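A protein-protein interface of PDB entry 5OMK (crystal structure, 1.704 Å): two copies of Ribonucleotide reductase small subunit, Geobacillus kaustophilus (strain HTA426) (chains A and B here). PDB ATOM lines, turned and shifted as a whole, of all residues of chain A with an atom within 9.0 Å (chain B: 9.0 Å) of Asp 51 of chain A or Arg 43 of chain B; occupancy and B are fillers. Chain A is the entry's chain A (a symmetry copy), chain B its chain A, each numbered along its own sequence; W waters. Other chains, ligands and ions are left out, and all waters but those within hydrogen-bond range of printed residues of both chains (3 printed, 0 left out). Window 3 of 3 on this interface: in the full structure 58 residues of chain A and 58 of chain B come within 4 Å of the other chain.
OD1 of Asn 48 of chain A sits at hydrogen-bond distance from NZ of Lys 42 of chain B (2.9 Å). NH2 of Arg 125 of chain A is in salt-bridge range of OE2 of Glu 39 of chain B (3.0 Å). NH1 of Arg 43 of chain B lies within salt-bridge range of OD1 of Asp 51 of chain A (2.8 Å). NZ of Lys 46 of chain A lies within hydrogen-bond range of O of Lys 46 of chain B. The side-chain carboxylate (OE2) of Glu 121 of chain A lies within hydrogen-bond range of the side-chain hydroxyl (OH) of Tyr 38 of chain B. NZ of Lys 42 of chain B lies within salt-bridge range of OE2 of Glu 121 of chain A, at 2.7 Å. The side-chain carboxylate (OE1) of Glu 121 of chain A lies close to the side-chain carboxylate (OE2) of Glu 39 of chain B (2.9 Å).
The side-chain amide oxygen (OD1) of Asn 48 of chain A sits at hydrogen-bond distance from the backbone NH (N) of Ala 50 of chain A, at 3.0 Å. The side-chain amino group (NZ) of Lys 42 of chain B lies within salt-bridge range of the side-chain carboxylate (OE2) of Glu 39 of chain B (2.6 Å). The side-chain amino group of Lys 46 of chain B is in hydrogen-bond range of the backbone carbonyl oxygen of Lys 42 of chain B. The guanidinium group (NE) of Arg 125 of chain A lies within salt-bridge range of the side-chain carboxylate (OE1) of Glu 121 of chain A (2.8 Å).
CZ of Arg 43 of chain B touches ND2 of Asn 48 of chain A, 3.7 Å away. CB of Ala 50 of chain A touches OE1 of Glu 39 of chain B, 3.5 Å away. NH2 of Arg 43 of chain B touches CB of Ala 50 of chain A (3.8 Å). CE1 of His 114 of chain A touches CE1 of Tyr 38 of chain B, 3.8 Å away. His 114 of chain A touches Lys 42 of chain B (CE1 to CG, 3.9 Å). Thr 111 of chain B touches His 114 of chain A (CG2 to CE1, 3.6 Å).
Of the printed residues of chain B, Lys 46 of chain A touches Lys 46 (3.2 Å). Of chain B, only Lys 42 (2.9 Å) and Arg 43 (3.7 Å) come within 4 Å of Asn 48 of chain A. Of chain B, only Arg 43 comes within 4 Å of Asp 51 of chain A. Of the printed residues of chain A, Tyr 38 of chain B touches His 114 and Glu 121. Of the printed residues of chain A, Lys 42 of chain B touches Asn 48, His 114 and Glu 121. Of chain A, only Asn 48, Ala 50 and Asp 51 come within 4 Å of Arg 43 of chain B. Trp 47 of chain B touches none of the printed residues of chain A. Of the printed residues of chain A, Thr 111 of chain B touches His 114. The nearest residue of chain B that does not touch Asp 51 of chain A is Lys 46 of chain B (6.7 Å).
Of the 16 printed residues of chain B, 6 touch a printed residue of chain A. Hydrophobic or aromatic side chains of chain B within 4 Å of the printed part of chain A: Tyr 38. Of the 17 printed residues of chain A, 7 touch a printed residue of chain B. Hydrophobic or aromatic side chains of chain A within 4 Å of the printed part of chain B: Ala 50 and His 114. Among the printed residues, 13 pairs touch across the chains. Among the printed residues, Asp or Glu carboxylates within 4 Å of a Lys or Arg side-chain nitrogen of the other chain: Asp 51 of chain A with Arg 43 of chain B, Glu 121 of chain A with Lys 42 of chain B and Arg 125 of chain A with Glu 39 of chain B.
Lys 46 of chain A touches its own counterpart, Lys 46 of chain B. Positions printed for both chains: 46 and 47.
Water W1 lies within hydrogen-bond range of the side-chain amino group (NZ) of Lys 46 of chain B (2.5 Å), the backbone carbonyl oxygen (O) of Trp 47 of chain A (3.0 Å) and the backbone carbonyl oxygen (O) of Lys 46 of chain A (3.4 Å). Water W2 lies within hydrogen-bond range of NZ of Lys 46 of chain A (2.5 Å), O of Trp 47 of chain B (3.0 Å) and O of Lys 46 of chain B (3.4 Å). Water W3 lies within hydrogen-bond range of OE1 of Glu 39 of chain B (2.7 Å), ND2 of Asn 48 of chain A (2.8 Å) and NE of Arg 43 of chain B (3.3 Å).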
ATOM      1  N   LYS A  46      29.555  -2.294  17.838  1.00  0.00           N
ATOM      2  CA  LYS A  46      29.387  -3.604  18.457  1.00  0.00           C
ATOM      3  C   LYS A  46      28.504  -3.558  19.706  1.00  0.00           C
ATOM      4  O   LYS A  46      28.135  -4.615  20.230  1.00  0.00           O
ATOM      5  CB  LYS A  46      30.743  -4.199  18.841  1.00  0.00           C
ATOM      6  CG  LYS A  46      31.702  -4.467  17.677  1.00  0.00           C
ATOM      7  CD  LYS A  46      31.065  -5.405  16.686  1.00  0.00           C
ATOM      8  CE  LYS A  46      32.120  -6.075  15.812  1.00  0.00           C
ATOM      9  NZ  LYS A  46      31.674  -6.117  14.402  1.00  0.00           N
ATOM     10  N   TRP A  47      28.167  -2.375  20.195  1.00  0.00           N
ATOM     11  CA  TRP A  47      27.438  -2.295  21.451  1.00  0.00           C
ATOM     12  C   TRP A  47      26.079  -2.971  21.323  1.00  0.00           C
ATOM     13  O   TRP A  47      25.452  -2.988  20.260  1.00  0.00           O
ATOM     14  CB  TRP A  47      27.287  -0.854  21.866  1.00  0.00           C
ATOM     15  CG  TRP A  47      26.267  -0.052  21.079  1.00  0.00           C
ATOM     16  CD1 TRP A  47      26.429   0.532  19.857  1.00  0.00           C
ATOM     17  CD2 TRP A  47      24.945   0.277  21.505  1.00  0.00           C
ATOM     18  NE1 TRP A  47      25.277   1.200  19.485  1.00  0.00           N
ATOM     19  CE2 TRP A  47      24.350   1.057  20.479  1.00  0.00           C
ATOM     20  CE3 TRP A  47      24.195  -0.022  22.650  1.00  0.00           C
ATOM     21  CZ2 TRP A  47      23.060   1.551  20.573  1.00  0.00           C
ATOM     22  CZ3 TRP A  47      22.910   0.467  22.742  1.00  0.00           C
ATOM     23  CH2 TRP A  47      22.355   1.255  21.699  1.00  0.00           C
ATOM     24  N   ASN A  48      25.615  -3.521  22.439  1.00  0.00           N
ATOM     25  CA  ASN A  48      24.376  -4.290  22.475  1.00  0.00           C
ATOM     26  C   ASN A  48      23.524  -3.712  23.600  1.00  0.00           C
ATOM     27  O   ASN A  48      23.966  -3.725  24.770  1.00  0.00           O
ATOM     28  CB  ASN A  48      24.656  -5.770  22.712  1.00  0.00           C
ATOM     29  CG  ASN A  48      23.407  -6.621  22.544  1.00  0.00           C
ATOM     30  OD1 ASN A  48      22.304  -6.114  22.642  1.00  0.00           O
ATOM     31  ND2 ASN A  48      23.578  -7.904  22.328  1.00  0.00           N
ATOM     32  N   PRO A  49      22.320  -3.189  23.308  1.00  0.00           N
ATOM     33  CA  PRO A  49      21.478  -2.630  24.372  1.00  0.00           C
ATOM     34  C   PRO A  49      21.189  -3.609  25.467  1.00  0.00           C
ATOM     35  O   PRO A  49      20.947  -3.182  26.607  1.00  0.00           O
ATOM     36  CB  PRO A  49      20.191  -2.247  23.632  1.00  0.00           C
ATOM     37  CG  PRO A  49      20.632  -2.071  22.188  1.00  0.00           C
ATOM     38  CD  PRO A  49      21.663  -3.114  21.994  1.00  0.00           C
ATOM     39  N   ALA A  50      21.144  -4.899  25.129  1.00  0.00           N
ATOM     40  CA  ALA A  50      20.923  -5.982  26.073  1.00  0.00           C
ATOM     41  C   ALA A  50      21.997  -6.080  27.152  1.00  0.00           C
ATOM     42  O   ALA A  50      21.790  -6.782  28.147  1.00  0.00           O
ATOM     43  CB  ALA A  50      20.860  -7.300  25.324  1.00  0.00           C
ATOM     44  N   ASP A  51      23.129  -5.433  26.972  1.00  0.00           N
ATOM     45  CA  ASP A  51      24.206  -5.492  27.946  1.00  0.00           C
ATOM     46  C   ASP A  51      24.155  -4.336  28.924  1.00  0.00           C
ATOM     47  O   ASP A  51      24.922  -4.333  29.894  1.00  0.00           O
ATOM     48  CB  ASP A  51      25.579  -5.483  27.260  1.00  0.00           C
ATOM     49  CG  ASP A  51      25.874  -6.749  26.480  1.00  0.00           C
ATOM     50  OD1 ASP A  51      25.336  -7.830  26.786  1.00  0.00           O
ATOM     51  OD2 ASP A  51      26.680  -6.649  25.548  1.00  0.00           O
ATOM     52  N   ILE A  52      23.289  -3.351  28.695  1.00  0.00           N
ATOM     53  CA  ILE A  52      23.228  -2.167  29.554  1.00  0.00           C
ATOM     54  C   ILE A  52      22.526  -2.534  30.854  1.00  0.00           C
ATOM     55  O   ILE A  52      21.474  -3.178  30.848  1.00  0.00           O
ATOM     56  CB  ILE A  52      22.493  -1.018  28.861  1.00  0.00           C
ATOM     57  CG1 ILE A  52      23.220  -0.601  27.579  1.00  0.00           C
ATOM     58  CG2 ILE A  52      22.376   0.193  29.789  1.00  0.00           C
ATOM     59  CD1 ILE A  52      22.498   0.514  26.835  1.00  0.00           C
ATOM     60  N   ASP A  53      23.117  -2.120  31.962  1.00  0.00           N
ATOM     61  CA  ASP A  53      22.583  -2.392  33.294  1.00  0.00           C
ATOM     62  C   ASP A  53      21.648  -1.241  33.647  1.00  0.00           C
ATOM     63  O   ASP A  53      22.089  -0.099  33.850  1.00  0.00           O
ATOM     64  CB  ASP A  53      23.733  -2.523  34.285  1.00  0.00           C
ATOM     65  CG  ASP A  53      23.270  -2.793  35.720  1.00  0.00           C
ATOM     66  OD1 ASP A  53      22.069  -3.003  35.939  1.00  0.00           O
ATOM     67  OD2 ASP A  53      24.139  -2.765  36.630  1.00  0.00           O
ATOM     68  N   PHE A  54      20.352  -1.522  33.662  1.00  0.00           N
ATOM     69  CA  PHE A  54      19.343  -0.527  33.975  1.00  0.00           C
ATOM     70  C   PHE A  54      18.867  -0.612  35.439  1.00  0.00           C
ATOM     71  O   PHE A  54      17.916   0.069  35.808  1.00  0.00           O
ATOM     72  CB  PHE A  54      18.146  -0.689  33.039  1.00  0.00           C
ATOM     73  CG  PHE A  54      18.415  -0.295  31.591  1.00  0.00           C
ATOM     74  CD1 PHE A  54      18.418  -1.245  30.579  1.00  0.00           C
ATOM     75  CD2 PHE A  54      18.635   1.032  31.260  1.00  0.00           C
ATOM     76  CE1 PHE A  54      18.650  -0.871  29.253  1.00  0.00           C
ATOM     77  CE2 PHE A  54      18.856   1.411  29.940  1.00  0.00           C
ATOM     78  CZ  PHE A  54      18.844   0.443  28.944  1.00  0.00           C
ATOM     79  N   SER A  55      19.501  -1.436  36.271  1.00  0.00           N
ATOM     80  CA  SER A  55      18.977  -1.642  37.621  1.00  0.00           C
ATOM     81  C   SER A  55      19.035  -0.362  38.434  1.00  0.00           C
ATOM     82  O   SER A  55      18.101  -0.058  39.189  1.00  0.00           O
ATOM     83  CB  SER A  55      19.726  -2.783  38.317  1.00  0.00           C
ATOM     84  OG  SER A  55      21.111  -2.507  38.415  1.00  0.00           O
ATOM     85  N   HIS A 114      20.390  -1.332  11.208  1.00  0.00           N
ATOM     86  CA  HIS A 114      20.610  -2.106  12.421  1.00  0.00           C
ATOM     87  C   HIS A 114      20.892  -1.206  13.620  1.00  0.00           C
ATOM     88  O   HIS A 114      20.420  -1.479  14.738  1.00  0.00           O
ATOM     89  CB  HIS A 114      21.750  -3.110  12.241  1.00  0.00           C
ATOM     90  CG  HIS A 114      21.957  -3.930  13.469  1.00  0.00           C
ATOM     91  ND1 HIS A 114      20.936  -4.687  14.005  1.00  0.00           N
ATOM     92  CD2 HIS A 114      23.017  -4.071  14.305  1.00  0.00           C
ATOM     93  CE1 HIS A 114      21.366  -5.284  15.107  1.00  0.00           C
ATOM     94  NE2 HIS A 114      22.624  -4.934  15.309  1.00  0.00           N
ATOM     95  N   GLU A 121      15.357  -0.544  20.535  1.00  0.00           N
ATOM     96  CA  GLU A 121      15.509  -1.517  21.616  1.00  0.00           C
ATOM     97  C   GLU A 121      15.967  -0.848  22.900  1.00  0.00           C
ATOM     98  O   GLU A 121      15.421  -1.117  23.969  1.00  0.00           O
ATOM     99  CB  GLU A 121      16.501  -2.601  21.213  1.00  0.00           C
ATOM    100  CG  GLU A 121      16.697  -3.712  22.261  1.00  0.00           C
ATOM    101  CD  GLU A 121      17.925  -4.554  22.028  1.00  0.00           C
ATOM    102  OE1 GLU A 121      18.303  -5.276  22.958  1.00  0.00           O
ATOM    103  OE2 GLU A 121      18.496  -4.515  20.917  1.00  0.00           O
ATOM    104  N   MET A 122      16.980   0.025  22.817  1.00  0.00           N
ATOM    105  CA  MET A 122      17.516   0.649  24.019  1.00  0.00           C
ATOM    106  C   MET A 122      16.431   1.411  24.782  1.00  0.00           C
ATOM    107  O   MET A 122      16.238   1.209  25.995  1.00  0.00           O
ATOM    108  CB  MET A 122      18.688   1.572  23.638  1.00  0.00           C
ATOM    109  CG  MET A 122      19.555   2.047  24.813  1.00  0.00           C
ATOM    110  SD  MET A 122      18.826   3.370  25.741  1.00  0.00           S
ATOM    111  CE  MET A 122      18.886   4.715  24.578  1.00  0.00           C
ATOM    112  N   ARG A 125      13.829  -0.895  26.265  1.00  0.00           N
ATOM    113  CA  ARG A 125      14.324  -1.614  27.444  1.00  0.00           C
ATOM    114  C   ARG A 125      14.335  -0.713  28.666  1.00  0.00           C
ATOM    115  O   ARG A 125      14.013  -1.158  29.779  1.00  0.00           O
ATOM    116  CB  ARG A 125      15.727  -2.165  27.216  1.00  0.00           C
ATOM    117  CG  ARG A 125      15.822  -3.445  26.437  1.00  0.00           C
ATOM    118  CD  ARG A 125      17.300  -3.904  26.327  1.00  0.00           C
ATOM    119  NE  ARG A 125      17.397  -5.141  25.573  1.00  0.00           N
ATOM    120  CZ  ARG A 125      17.195  -6.360  26.048  1.00  0.00           C
ATOM    121  NH1 ARG A 125      16.894  -6.567  27.332  1.00  0.00           N
ATOM    122  NH2 ARG A 125      17.283  -7.388  25.211  1.00  0.00           N
ATOM    123  N   GLY A 204      22.180   4.058  33.124  1.00  0.00           N
ATOM    124  CA  GLY A 204      22.015   3.155  31.993  1.00  0.00           C
ATOM    125  C   GLY A 204      21.498   3.876  30.765  1.00  0.00           C
ATOM    126  O   GLY A 204      22.023   3.709  29.660  1.00  0.00           O
ATOM    127  N   GLN A 207      24.335   5.920  29.315  1.00  0.00           N
ATOM    128  CA  GLN A 207      25.231   5.059  28.537  1.00  0.00           C
ATOM    129  C   GLN A 207      24.650   4.801  27.146  1.00  0.00           C
ATOM    130  O   GLN A 207      25.331   4.930  26.115  1.00  0.00           O
ATOM    131  CB  GLN A 207      25.445   3.755  29.292  1.00  0.00           C
ATOM    132  CG  GLN A 207      26.338   2.770  28.590  1.00  0.00           C
ATOM    133  CD  GLN A 207      26.703   1.603  29.475  1.00  0.00           C
ATOM    134  OE1 GLN A 207      25.842   0.990  30.116  1.00  0.00           O
ATOM    135  NE2 GLN A 207      27.988   1.306  29.541  1.00  0.00           N
ATOM    136  N   TYR A 211      26.114   5.836  23.278  1.00  0.00           N
ATOM    137  CA  TYR A 211      26.202   4.956  22.122  1.00  0.00           C
ATOM    138  C   TYR A 211      25.378   5.482  20.957  1.00  0.00           C
ATOM    139  O   TYR A 211      25.807   5.396  19.803  1.00  0.00           O
ATOM    140  CB  TYR A 211      25.729   3.559  22.476  1.00  0.00           C
ATOM    141  CG  TYR A 211      26.624   2.760  23.399  1.00  0.00           C
ATOM    142  CD1 TYR A 211      27.965   2.558  23.121  1.00  0.00           C
ATOM    143  CD2 TYR A 211      26.079   2.134  24.519  1.00  0.00           C
ATOM    144  CE1 TYR A 211      28.767   1.783  23.982  1.00  0.00           C
ATOM    145  CE2 TYR A 211      26.841   1.373  25.359  1.00  0.00           C
ATOM    146  CZ  TYR A 211      28.183   1.190  25.097  1.00  0.00           C
ATOM    147  OH  TYR A 211      28.903   0.396  25.975  1.00  0.00           O
ATOM    148  N   LYS B  36      13.626 -12.833  19.747  1.00  0.00           N
ATOM    149  CA  LYS B  36      14.615 -13.752  20.285  1.00  0.00           C
ATOM    150  C   LYS B  36      15.701 -14.027  19.247  1.00  0.00           C
ATOM    151  O   LYS B  36      16.902 -14.040  19.563  1.00  0.00           O
ATOM    152  CB  LYS B  36      13.916 -15.033  20.720  1.00  0.00           C
ATOM    153  CG  LYS B  36      13.114 -14.803  22.056  1.00  0.00           C
ATOM    154  CD  LYS B  36      12.622 -16.051  22.721  1.00  0.00           C
ATOM    155  CE  LYS B  36      12.780 -15.943  24.251  1.00  0.00           C
ATOM    156  NZ  LYS B  36      12.446 -14.584  24.803  1.00  0.00           N
ATOM    157  N   LEU B  37      15.289 -14.220  17.999  1.00  0.00           N
ATOM    158  CA  LEU B  37      16.255 -14.464  16.927  1.00  0.00           C
ATOM    159  C   LEU B  37      17.155 -13.248  16.678  1.00  0.00           C
ATOM    160  O   LEU B  37      18.364 -13.396  16.439  1.00  0.00           O
ATOM    161  CB  LEU B  37      15.502 -14.858  15.672  1.00  0.00           C
ATOM    162  CG  LEU B  37      16.338 -15.500  14.579  1.00  0.00           C
ATOM    163  CD1 LEU B  37      16.940 -16.841  15.046  1.00  0.00           C
ATOM    164  CD2 LEU B  37      15.478 -15.681  13.370  1.00  0.00           C
ATOM    165  N   TYR B  38      16.572 -12.048  16.693  1.00  0.00           N
ATOM    166  CA  TYR B  38      17.346 -10.811  16.662  1.00  0.00           C
ATOM    167  C   TYR B  38      18.404 -10.790  17.758  1.00  0.00           C
ATOM    168  O   TYR B  38      19.546 -10.389  17.527  1.00  0.00           O
ATOM    169  CB  TYR B  38      16.373  -9.648  16.814  1.00  0.00           C
ATOM    170  CG  TYR B  38      16.910  -8.297  17.197  1.00  0.00           C
ATOM    171  CD1 TYR B  38      17.538  -7.480  16.252  1.00  0.00           C
ATOM    172  CD2 TYR B  38      16.733  -7.774  18.495  1.00  0.00           C
ATOM    173  CE1 TYR B  38      17.978  -6.197  16.578  1.00  0.00           C
ATOM    174  CE2 TYR B  38      17.173  -6.511  18.815  1.00  0.00           C
ATOM    175  CZ  TYR B  38      17.808  -5.733  17.846  1.00  0.00           C
ATOM    176  OH  TYR B  38      18.237  -4.498  18.152  1.00  0.00           O
ATOM    177  N   GLU B  39      18.023 -11.184  18.974  1.00  0.00           N
ATOM    178  CA  GLU B  39      18.967 -11.175  20.084  1.00  0.00           C
ATOM    179  C   GLU B  39      20.100 -12.154  19.829  1.00  0.00           C
ATOM    180  O   GLU B  39      21.272 -11.839  20.073  1.00  0.00           O
ATOM    181  CB  GLU B  39      18.226 -11.495  21.388  1.00  0.00           C
ATOM    182  CG  GLU B  39      17.397 -10.319  21.913  1.00  0.00           C
ATOM    183  CD  GLU B  39      18.240  -9.262  22.599  1.00  0.00           C
ATOM    184  OE1 GLU B  39      19.173  -9.617  23.315  1.00  0.00           O
ATOM    185  OE2 GLU B  39      17.999  -8.063  22.419  1.00  0.00           O
ATOM    186  N   LYS B  40      19.774 -13.329  19.288  1.00  0.00           N
ATOM    187  CA  LYS B  40      20.803 -14.321  18.972  1.00  0.00           C
ATOM    188  C   LYS B  40      21.704 -13.824  17.855  1.00  0.00           C
ATOM    189  O   LYS B  40      22.915 -14.059  17.876  1.00  0.00           O
ATOM    190  CB  LYS B  40      20.179 -15.652  18.551  1.00  0.00           C
ATOM    191  CG  LYS B  40      19.535 -16.458  19.647  1.00  0.00           C
ATOM    192  CD  LYS B  40      18.616 -17.539  19.067  1.00  0.00           C
ATOM    193  CE  LYS B  40      17.134 -17.365  19.508  1.00  0.00           C
ATOM    194  NZ  LYS B  40      16.112 -17.749  18.450  1.00  0.00           N
ATOM    195  N   ALA B  41      21.129 -13.096  16.896  1.00  0.00           N
ATOM    196  CA  ALA B  41      21.934 -12.551  15.799  1.00  0.00           C
ATOM    197  C   ALA B  41      22.952 -11.534  16.304  1.00  0.00           C
ATOM    198  O   ALA B  41      24.099 -11.494  15.817  1.00  0.00           O
ATOM    199  CB  ALA B  41      21.007 -11.925  14.755  1.00  0.00           C
ATOM    200  N   LYS B  42      22.556 -10.672  17.250  1.00  0.00           N
ATOM    201  CA  LYS B  42      23.517  -9.732  17.835  1.00  0.00           C
ATOM    202  C   LYS B  42      24.642 -10.476  18.543  1.00  0.00           C
ATOM    203  O   LYS B  42      25.824 -10.138  18.396  1.00  0.00           O
ATOM    204  CB  LYS B  42      22.830  -8.766  18.806  1.00  0.00           C
ATOM    205  CG  LYS B  42      21.959  -7.719  18.151  1.00  0.00           C
ATOM    206  CD  LYS B  42      21.321  -6.813  19.176  1.00  0.00           C
ATOM    207  CE  LYS B  42      20.293  -7.574  19.986  1.00  0.00           C
ATOM    208  NZ  LYS B  42      19.910  -6.794  21.174  1.00  0.00           N
ATOM    209  N   ARG B  43      24.298 -11.512  19.293  1.00  0.00           N
ATOM    210  CA  ARG B  43      25.309 -12.217  20.071  1.00  0.00           C
ATOM    211  C   ARG B  43      26.262 -12.998  19.182  1.00  0.00           C
ATOM    212  O   ARG B  43      27.453 -13.064  19.474  1.00  0.00           O
ATOM    213  CB  ARG B  43      24.633 -13.167  21.064  1.00  0.00           C
ATOM    214  CG  ARG B  43      23.814 -12.463  22.061  1.00  0.00           C
ATOM    215  CD  ARG B  43      24.705 -11.926  23.149  1.00  0.00           C
ATOM    216  NE  ARG B  43      23.906 -11.358  24.223  1.00  0.00           N
ATOM    217  CZ  ARG B  43      24.319 -10.375  25.013  1.00  0.00           C
ATOM    218  NH1 ARG B  43      25.518  -9.846  24.861  1.00  0.00           N
ATOM    219  NH2 ARG B  43      23.515  -9.903  25.950  1.00  0.00           N
ATOM    220  N   ASN B  44      25.756 -13.599  18.107  1.00  0.00           N
ATOM    221  CA  ASN B  44      26.492 -14.530  17.283  1.00  0.00           C
ATOM    222  C   ASN B  44      26.951 -13.900  15.978  1.00  0.00           C
ATOM    223  O   ASN B  44      27.555 -14.593  15.159  1.00  0.00           O
ATOM    224  CB  ASN B  44      25.634 -15.775  16.930  1.00  0.00           C
ATOM    225  CG  ASN B  44      25.233 -16.621  18.141  1.00  0.00           C
ATOM    226  OD1 ASN B  44      25.811 -16.522  19.207  1.00  0.00           O
ATOM    227  ND2 ASN B  44      24.197 -17.433  17.968  1.00  0.00           N
ATOM    228  N   GLY B  45      26.687 -12.612  15.769  1.00  0.00           N
ATOM    229  CA  GLY B  45      26.959 -11.971  14.492  1.00  0.00           C
ATOM    230  C   GLY B  45      28.042 -10.917  14.534  1.00  0.00           C
ATOM    231  O   GLY B  45      27.968  -9.933  13.796  1.00  0.00           O
ATOM    232  N   LYS B  46      29.066 -11.097  15.367  1.00  0.00           N
ATOM    233  CA  LYS B  46      30.070 -10.051  15.523  1.00  0.00           C
ATOM    234  C   LYS B  46      31.219 -10.180  14.520  1.00  0.00           C
ATOM    235  O   LYS B  46      32.048  -9.269  14.422  1.00  0.00           O
ATOM    236  CB  LYS B  46      30.655 -10.068  16.937  1.00  0.00           C
ATOM    237  CG  LYS B  46      29.660  -9.789  18.068  1.00  0.00           C
ATOM    238  CD  LYS B  46      29.011  -8.445  17.867  1.00  0.00           C
ATOM    239  CE  LYS B  46      28.423  -7.923  19.173  1.00  0.00           C
ATOM    240  NZ  LYS B  46      27.092  -7.319  18.937  1.00  0.00           N
ATOM    241  N   TRP B  47      31.293 -11.280  13.788  1.00  0.00           N
ATOM    242  CA  TRP B  47      32.440 -11.492  12.919  1.00  0.00           C
ATOM    243  C   TRP B  47      32.508 -10.409  11.851  1.00  0.00           C
ATOM    244  O   TRP B  47      31.495  -9.874  11.393  1.00  0.00           O
ATOM    245  CB  TRP B  47      32.365 -12.862  12.295  1.00  0.00           C
ATOM    246  CG  TRP B  47      31.340 -13.019  11.186  1.00  0.00           C
ATOM    247  CD1 TRP B  47      29.999 -13.231  11.316  1.00  0.00           C
ATOM    248  CD2 TRP B  47      31.609 -13.015   9.785  1.00  0.00           C
ATOM    249  NE1 TRP B  47      29.407 -13.348  10.072  1.00  0.00           N
ATOM    250  CE2 TRP B  47      30.374 -13.218   9.116  1.00  0.00           C
ATOM    251  CE3 TRP B  47      32.773 -12.847   9.024  1.00  0.00           C
ATOM    252  CZ2 TRP B  47      30.276 -13.273   7.736  1.00  0.00           C
ATOM    253  CZ3 TRP B  47      32.675 -12.899   7.650  1.00  0.00           C
ATOM    254  CH2 TRP B  47      31.422 -13.117   7.018  1.00  0.00           C
ATOM    255  N   THR B 111      19.390  -7.470  11.082  1.00  0.00           N
ATOM    256  CA  THR B 111      20.576  -8.308  11.227  1.00  0.00           C
ATOM    257  C   THR B 111      20.763  -9.191  10.001  1.00  0.00           C
ATOM    258  O   THR B 111      21.896  -9.420   9.555  1.00  0.00           O
ATOM    259  CB  THR B 111      20.526  -9.181  12.505  1.00  0.00           C
ATOM    260  OG1 THR B 111      19.584 -10.256  12.375  1.00  0.00           O
ATOM    261  CG2 THR B 111      20.235  -8.353  13.711  1.00  0.00           C
ATOM    262  N   MET B 214      26.905 -20.324   9.761  1.00  0.00           N
ATOM    263  CA  MET B 214      26.291 -19.995  11.051  1.00  0.00           C
ATOM    264  C   MET B 214      25.220 -18.916  10.915  1.00  0.00           C
ATOM    265  O   MET B 214      24.141 -19.016  11.507  1.00  0.00           O
ATOM    266  CB  MET B 214      27.330 -19.493  12.044  1.00  0.00           C
ATOM    267  CG  MET B 214      28.190 -20.518  12.729  1.00  0.00           C
ATOM    268  SD  MET B 214      29.275 -19.619  13.885  1.00  0.00           S
ATOM    269  CE  MET B 214      28.074 -18.752  14.914  1.00  0.00           C
ATOM    270  N   ASP B 215      25.524 -17.841  10.191  1.00  0.00           N
ATOM    271  CA  ASP B 215      24.497 -16.844   9.928  1.00  0.00           C
ATOM    272  C   ASP B 215      23.278 -17.474   9.261  1.00  0.00           C
ATOM    273  O   ASP B 215      22.137 -17.103   9.562  1.00  0.00           O
ATOM    274  CB  ASP B 215      25.033 -15.721   9.034  1.00  0.00           C
ATOM    275  CG  ASP B 215      26.129 -14.892   9.678  1.00  0.00           C
ATOM    276  OD1 ASP B 215      26.247 -14.815  10.917  1.00  0.00           O
ATOM    277  OD2 ASP B 215      26.890 -14.283   8.900  1.00  0.00           O
ATOM    278  N   ARG B 218      20.031 -18.633  11.031  1.00  0.00           N
ATOM    279  CA  ARG B 218      19.005 -17.665  11.415  1.00  0.00           C
ATOM    280  C   ARG B 218      18.152 -17.267  10.222  1.00  0.00           C
ATOM    281  O   ARG B 218      16.945 -17.096  10.361  1.00  0.00           O
ATOM    282  CB  ARG B 218      19.640 -16.441  12.068  1.00  0.00           C
ATOM    283  CG  ARG B 218      20.496 -16.714  13.310  1.00  0.00           C
ATOM    284  CD  ARG B 218      20.895 -15.417  13.964  1.00  0.00           C
ATOM    285  NE  ARG B 218      21.774 -14.650  13.085  1.00  0.00           N
ATOM    286  CZ  ARG B 218      23.075 -14.852  12.987  1.00  0.00           C
ATOM    287  NH1 ARG B 218      23.671 -15.814  13.707  1.00  0.00           N
ATOM    288  NH2 ARG B 218      23.781 -14.131  12.132  1.00  0.00           N
HETATM  289  O   HOH W   1      25.100  -5.769  19.289  1.00  0.00           O
HETATM  290  O   HOH W   2      31.464  -6.972  12.010  1.00  0.00           O
HETATM  291  O   HOH W   3      21.643  -9.897  22.251  1.00  0.00           O
